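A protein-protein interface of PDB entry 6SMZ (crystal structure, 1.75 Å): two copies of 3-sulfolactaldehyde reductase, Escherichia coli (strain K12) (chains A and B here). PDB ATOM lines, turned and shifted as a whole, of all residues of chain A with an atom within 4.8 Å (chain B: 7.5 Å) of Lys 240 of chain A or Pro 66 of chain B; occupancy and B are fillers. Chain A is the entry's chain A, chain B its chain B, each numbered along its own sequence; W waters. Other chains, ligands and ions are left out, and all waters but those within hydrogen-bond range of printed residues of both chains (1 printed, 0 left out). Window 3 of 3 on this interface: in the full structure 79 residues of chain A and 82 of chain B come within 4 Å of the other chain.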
ATOM      1  N   ASP A 236       0.518  14.736 -16.258  1.00  0.00           N
ATOM      2  CA  ASP A 236      -0.284  13.634 -15.666  1.00  0.00           C
ATOM      3  C   ASP A 236      -1.237  13.018 -16.691  1.00  0.00           C
ATOM      4  O   ASP A 236      -1.333  11.787 -16.704  1.00  0.00           O
ATOM      5  CB  ASP A 236      -1.048  14.089 -14.426  1.00  0.00           C
ATOM      6  CG  ASP A 236      -0.202  14.337 -13.204  1.00  0.00           C
ATOM      7  OD1 ASP A 236       0.913  13.783 -13.066  1.00  0.00           O
ATOM      8  OD2 ASP A 236      -0.682  15.128 -12.335  1.00  0.00           O
ATOM      9  N   LEU A 237      -1.956  13.807 -17.501  1.00  0.00           N
ATOM     10  CA  LEU A 237      -2.934  13.247 -18.463  1.00  0.00           C
ATOM     11  C   LEU A 237      -2.182  12.573 -19.615  1.00  0.00           C
ATOM     12  O   LEU A 237      -2.651  11.495 -20.091  1.00  0.00           O
ATOM     13  CB  LEU A 237      -3.871  14.336 -18.994  1.00  0.00           C
ATOM     14  N   ALA A 238      -1.084  13.180 -20.080  1.00  0.00           N
ATOM     15  CA  ALA A 238      -0.243  12.579 -21.153  1.00  0.00           C
ATOM     16  C   ALA A 238       0.246  11.204 -20.671  1.00  0.00           C
ATOM     17  O   ALA A 238       0.133  10.218 -21.420  1.00  0.00           O
ATOM     18  CB  ALA A 238       0.891  13.508 -21.492  1.00  0.00           C
ATOM     19  N   HIS A 239       0.732  11.140 -19.439  1.00  0.00           N
ATOM     20  CA  HIS A 239       1.256   9.886 -18.816  1.00  0.00           C
ATOM     21  C   HIS A 239       0.136   8.850 -18.762  1.00  0.00           C
ATOM     22  O   HIS A 239       0.356   7.692 -19.093  1.00  0.00           O
ATOM     23  CB  HIS A 239       1.904  10.214 -17.480  1.00  0.00           C
ATOM     24  CG  HIS A 239       2.331   9.018 -16.718  1.00  0.00           C
ATOM     25  ND1 HIS A 239       1.542   8.466 -15.702  1.00  0.00           N
ATOM     26  CD2 HIS A 239       3.472   8.282 -16.788  1.00  0.00           C
ATOM     27  CE1 HIS A 239       2.188   7.420 -15.204  1.00  0.00           C
ATOM     28  NE2 HIS A 239       3.356   7.257 -15.876  1.00  0.00           N
ATOM     29  N   LYS A 240      -1.088   9.262 -18.398  1.00  0.00           N
ATOM     30  CA  LYS A 240      -2.236   8.330 -18.290  1.00  0.00           C
ATOM     31  C   LYS A 240      -2.568   7.776 -19.671  1.00  0.00           C
ATOM     32  O   LYS A 240      -2.747   6.524 -19.779  1.00  0.00           O
ATOM     33  CB  LYS A 240      -3.437   9.050 -17.645  1.00  0.00           C
ATOM     34  CG  LYS A 240      -4.811   8.369 -17.741  1.00  0.00           C
ATOM     35  CD  LYS A 240      -6.004   9.382 -17.617  1.00  0.00           C
ATOM     36  CE  LYS A 240      -7.354   8.782 -17.951  1.00  0.00           C
ATOM     37  N   ASP A 241      -2.702   8.631 -20.695  1.00  0.00           N
ATOM     38  CA  ASP A 241      -3.093   8.208 -22.059  1.00  0.00           C
ATOM     39  C   ASP A 241      -2.011   7.264 -22.618  1.00  0.00           C
ATOM     40  O   ASP A 241      -2.353   6.287 -23.299  1.00  0.00           O
ATOM     41  CB  ASP A 241      -3.316   9.399 -22.998  1.00  0.00           C
ATOM     42  CG  ASP A 241      -4.656  10.095 -22.823  1.00  0.00           C
ATOM     43  OD1 ASP A 241      -5.422   9.664 -21.891  1.00  0.00           O
ATOM     44  OD2 ASP A 241      -4.929  11.025 -23.658  1.00  0.00           O
ATOM     45  N   LEU A 242      -0.745   7.544 -22.346  1.00  0.00           N
ATOM     46  CA  LEU A 242       0.377   6.680 -22.801  1.00  0.00           C
ATOM     47  C   LEU A 242       0.272   5.301 -22.126  1.00  0.00           C
ATOM     48  O   LEU A 242       0.499   4.286 -22.793  1.00  0.00           O
ATOM     49  CB  LEU A 242       1.639   7.448 -22.436  1.00  0.00           C
ATOM     50  CG  LEU A 242       2.963   6.899 -22.909  1.00  0.00           C
ATOM     51  CD1 LEU A 242       2.921   6.620 -24.398  1.00  0.00           C
ATOM     52  CD2 LEU A 242       4.046   7.932 -22.566  1.00  0.00           C
ATOM     53  N   GLY A 243      -0.103   5.248 -20.853  1.00  0.00           N
ATOM     54  CA  GLY A 243      -0.397   3.984 -20.152  1.00  0.00           C
ATOM     55  C   GLY A 243      -1.485   3.190 -20.850  1.00  0.00           C
ATOM     56  O   GLY A 243      -1.294   1.973 -21.054  1.00  0.00           O
ATOM     57  N   ILE A 244      -2.587   3.823 -21.248  1.00  0.00           N
ATOM     58  CA  ILE A 244      -3.667   3.130 -21.985  1.00  0.00           C
ATOM     59  C   ILE A 244      -3.109   2.581 -23.308  1.00  0.00           C
ATOM     60  O   ILE A 244      -3.401   1.438 -23.635  1.00  0.00           O
ATOM     61  CB  ILE A 244      -4.879   4.059 -22.234  1.00  0.00           C
ATOM     62  CG1 ILE A 244      -5.469   4.596 -20.933  1.00  0.00           C
ATOM     63  CG2 ILE A 244      -5.920   3.329 -23.058  1.00  0.00           C
ATOM     64  CD1 ILE A 244      -6.479   5.724 -21.179  1.00  0.00           C
ATOM     65  N   GLY B   8     -20.740  14.927 -16.503  1.00  0.00           N
ATOM     66  CA  GLY B   8     -19.291  15.215 -16.464  1.00  0.00           C
ATOM     67  C   GLY B   8     -19.044  16.645 -16.852  1.00  0.00           C
ATOM     68  O   GLY B   8     -19.017  16.929 -18.073  1.00  0.00           O
ATOM     69  N   MET B  64     -18.651  13.010 -20.420  1.00  0.00           N
ATOM     70  CA  MET B  64     -17.279  13.544 -20.543  1.00  0.00           C
ATOM     71  C   MET B  64     -16.557  13.271 -19.220  1.00  0.00           C
ATOM     72  O   MET B  64     -16.584  14.139 -18.346  1.00  0.00           O
ATOM     73  CB  MET B  64     -17.284  15.031 -20.898  1.00  0.00           C
ATOM     74  CG  MET B  64     -15.921  15.560 -21.333  1.00  0.00           C
ATOM     75  SD  MET B  64     -15.211  14.529 -22.647  1.00  0.00           S
ATOM     76  CE  MET B  64     -13.956  15.643 -23.269  1.00  0.00           C
ATOM     77  N   LEU B  65     -15.980  12.062 -19.107  1.00  0.00           N
ATOM     78  CA  LEU B  65     -15.558  11.523 -17.788  1.00  0.00           C
ATOM     79  C   LEU B  65     -14.103  11.055 -17.855  1.00  0.00           C
ATOM     80  O   LEU B  65     -13.582  10.817 -18.937  1.00  0.00           O
ATOM     81  CB  LEU B  65     -16.501  10.384 -17.418  1.00  0.00           C
ATOM     82  CG  LEU B  65     -17.940  10.823 -17.116  1.00  0.00           C
ATOM     83  CD1 LEU B  65     -18.865   9.618 -17.073  1.00  0.00           C
ATOM     84  CD2 LEU B  65     -18.015  11.561 -15.796  1.00  0.00           C
ATOM     85  N   PRO B  66     -13.408  10.964 -16.709  1.00  0.00           N
ATOM     86  CA  PRO B  66     -11.989  10.576 -16.703  1.00  0.00           C
ATOM     87  C   PRO B  66     -11.637   9.176 -17.240  1.00  0.00           C
ATOM     88  O   PRO B  66     -10.522   9.050 -17.747  1.00  0.00           O
ATOM     89  CB  PRO B  66     -11.612  10.701 -15.220  1.00  0.00           C
ATOM     90  CG  PRO B  66     -12.627  11.660 -14.632  1.00  0.00           C
ATOM     91  CD  PRO B  66     -13.907  11.307 -15.366  1.00  0.00           C
ATOM     92  N   ASN B  67     -12.502   8.169 -17.122  1.00  0.00           N
ATOM     93  CA  ASN B  67     -12.113   6.784 -17.504  1.00  0.00           C
ATOM     94  C   ASN B  67     -13.329   5.909 -17.806  1.00  0.00           C
ATOM     95  O   ASN B  67     -14.469   6.290 -17.495  1.00  0.00           O
ATOM     96  CB  ASN B  67     -11.203   6.181 -16.431  1.00  0.00           C
ATOM     97  CG  ASN B  67     -11.947   5.915 -15.140  1.00  0.00           C
ATOM     98  OD1 ASN B  67     -12.932   5.178 -15.145  1.00  0.00           O
ATOM     99  ND2 ASN B  67     -11.508   6.514 -14.055  1.00  0.00           N
ATOM    100  N   GLY B  68     -13.081   4.756 -18.416  1.00  0.00           N
ATOM    101  CA  GLY B  68     -14.123   3.836 -18.902  1.00  0.00           C
ATOM    102  C   GLY B  68     -14.925   3.198 -17.782  1.00  0.00           C
ATOM    103  O   GLY B  68     -16.087   2.824 -18.044  1.00  0.00           O
ATOM    104  N   ASP B  69     -14.327   3.022 -16.601  1.00  0.00           N
ATOM    105  CA  ASP B  69     -15.059   2.466 -15.431  1.00  0.00           C
ATOM    106  C   ASP B  69     -16.157   3.456 -15.021  1.00  0.00           C
ATOM    107  O   ASP B  69     -17.290   3.007 -14.771  1.00  0.00           O
ATOM    108  CB  ASP B  69     -14.101   2.151 -14.280  1.00  0.00           C
ATOM    109  CG  ASP B  69     -13.099   1.069 -14.609  1.00  0.00           C
ATOM    110  OD1 ASP B  69     -13.489   0.152 -15.361  1.00  0.00           O
ATOM    111  OD2 ASP B  69     -11.955   1.171 -14.127  1.00  0.00           O
ATOM    112  N   LEU B  70     -15.835   4.755 -14.995  1.00  0.00           N
ATOM    113  CA  LEU B  70     -16.816   5.809 -14.627  1.00  0.00           C
ATOM    114  C   LEU B  70     -17.883   5.921 -15.724  1.00  0.00           C
ATOM    115  O   LEU B  70     -19.071   6.027 -15.386  1.00  0.00           O
ATOM    116  CB  LEU B  70     -16.087   7.131 -14.375  1.00  0.00           C
ATOM    117  CG  LEU B  70     -15.194   7.154 -13.140  1.00  0.00           C
ATOM    118  CD1 LEU B  70     -14.437   8.466 -13.051  1.00  0.00           C
ATOM    119  CD2 LEU B  70     -16.009   6.915 -11.894  1.00  0.00           C
ATOM    120  N   VAL B  71     -17.521   5.830 -16.999  1.00  0.00           N
ATOM    121  CA  VAL B  71     -18.551   5.841 -18.074  1.00  0.00           C
ATOM    122  C   VAL B  71     -19.490   4.641 -17.856  1.00  0.00           C
ATOM    123  O   VAL B  71     -20.728   4.831 -17.904  1.00  0.00           O
ATOM    124  CB  VAL B  71     -17.940   5.829 -19.480  1.00  0.00           C
ATOM    125  CG1 VAL B  71     -19.030   5.725 -20.540  1.00  0.00           C
ATOM    126  CG2 VAL B  71     -17.068   7.055 -19.691  1.00  0.00           C
ATOM    127  N   SER B  95     -15.505  10.945 -23.889  1.00  0.00           N
ATOM    128  CA  SER B  95     -14.354  10.611 -23.003  1.00  0.00           C
ATOM    129  C   SER B  95     -13.228   9.962 -23.806  1.00  0.00           C
ATOM    130  O   SER B  95     -13.503   9.303 -24.831  1.00  0.00           O
ATOM    131  CB  SER B  95     -14.787   9.701 -21.868  1.00  0.00           C
ATOM    132  OG  SER B  95     -15.967  10.182 -21.230  1.00  0.00           O
ATOM    133  N   THR B  96     -11.991  10.089 -23.315  1.00  0.00           N
ATOM    134  CA  THR B  96     -10.849   9.295 -23.839  1.00  0.00           C
ATOM    135  C   THR B  96     -10.678   8.090 -22.923  1.00  0.00           C
ATOM    136  O   THR B  96     -10.199   8.270 -21.814  1.00  0.00           O
ATOM    137  CB  THR B  96      -9.574  10.137 -23.950  1.00  0.00           C
ATOM    138  OG1 THR B  96      -9.849  11.202 -24.851  1.00  0.00           O
ATOM    139  CG2 THR B  96      -8.410   9.325 -24.469  1.00  0.00           C
ATOM    140  N   ILE B  97     -11.111   6.921 -23.367  1.00  0.00           N
ATOM    141  CA  ILE B  97     -11.067   5.660 -22.579  1.00  0.00           C
ATOM    142  C   ILE B  97     -10.431   4.566 -23.429  1.00  0.00           C
ATOM    143  O   ILE B  97     -10.138   4.770 -24.621  1.00  0.00           O
ATOM    144  CB  ILE B  97     -12.492   5.274 -22.090  1.00  0.00           C
ATOM    145  CG1 ILE B  97     -13.423   4.868 -23.239  1.00  0.00           C
ATOM    146  CG2 ILE B  97     -13.086   6.416 -21.276  1.00  0.00           C
ATOM    147  CD1 ILE B  97     -14.706   4.209 -22.776  1.00  0.00           C
ATOM    148  N   LEU B 172      -6.724   7.504 -29.787  1.00  0.00           N
ATOM    149  CA  LEU B 172      -5.613   6.802 -29.090  1.00  0.00           C
ATOM    150  C   LEU B 172      -4.350   6.848 -29.972  1.00  0.00           C
ATOM    151  O   LEU B 172      -3.245   7.135 -29.428  1.00  0.00           O
ATOM    152  CB  LEU B 172      -6.037   5.371 -28.770  1.00  0.00           C
ATOM    153  CG  LEU B 172      -4.972   4.584 -27.985  1.00  0.00           C
ATOM    154  CD1 LEU B 172      -4.686   5.272 -26.659  1.00  0.00           C
ATOM    155  CD2 LEU B 172      -5.400   3.155 -27.754  1.00  0.00           C
ATOM    156  N   ILE B 179       2.247  12.086 -27.837  1.00  0.00           N
ATOM    157  CA  ILE B 179       2.795  12.079 -26.454  1.00  0.00           C
ATOM    158  C   ILE B 179       4.221  11.505 -26.538  1.00  0.00           C
ATOM    159  O   ILE B 179       5.103  12.080 -25.943  1.00  0.00           O
ATOM    160  CB  ILE B 179       1.903  11.280 -25.508  1.00  0.00           C
ATOM    161  CG1 ILE B 179       0.552  11.987 -25.348  1.00  0.00           C
ATOM    162  CG2 ILE B 179       2.546  11.114 -24.166  1.00  0.00           C
ATOM    163  CD1 ILE B 179      -0.538  11.142 -24.760  1.00  0.00           C
HETATM  164  O   HOH W   1      -7.260  12.629 -23.881  1.00  0.00           O
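Water W1 lies within hydrogen-bond range of the side-chain carboxylate (OD2) of Asp 241 of chain A (2.8 Å) and the side-chain hydroxyl (OG1) of Thr 96 of chain B (3.1 Å).
No position is printed for both chains. Of the 5 pairs that touch across the chains among the printed residues, none has its exchanged pair printed and touching as well.
Among the printed residues, pairs that only touch across the chains: Ala 238 of chain A with Ile 179 of chain B (3.5 Å), Lys 240 of chain A with Pro 66 of chain B (3.2 Å), Asp 241 of chain A with Thr 96 of chain B (3.96 Å), Asp 241 of chain A with Ile 179 of chain B (3.7 Å) and Leu 242 of chain A with Ile 179 of chain B (3.9 Å).
Printed residues of chain B that touch a printed residue of chain A: Pro 66, Thr 96 and Ile 179. Hydrophobic or aromatic side chains of chain B that line the printed part of chain A: Ile 179. Printed residues of chain A that touch a printed residue of chain B: Ala 238, Lys 240, Asp 241 and Leu 242. Among the printed residues, 5 pairs touch across the chains.
Lys 240 of chain A touches just one residue of chain B: Pro 66 (3.2 Å). Of the printed residues of chain B, Leu 242 of chain A touches Ile 179 (3.9 Å). Of the printed residues of chain B, Ala 238 of chain A touches Ile 179. Of the printed residues of chain B, Asp 241 of chain A touches Thr 96 (3.96 Å) and Ile 179 (3.7 Å). Ile 97 of chain B touches none of the printed residues of chain A. The nearest printed residue of chain B that does not touch Leu 242 of chain A is Leu 172 of chain B (6.3 Å).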
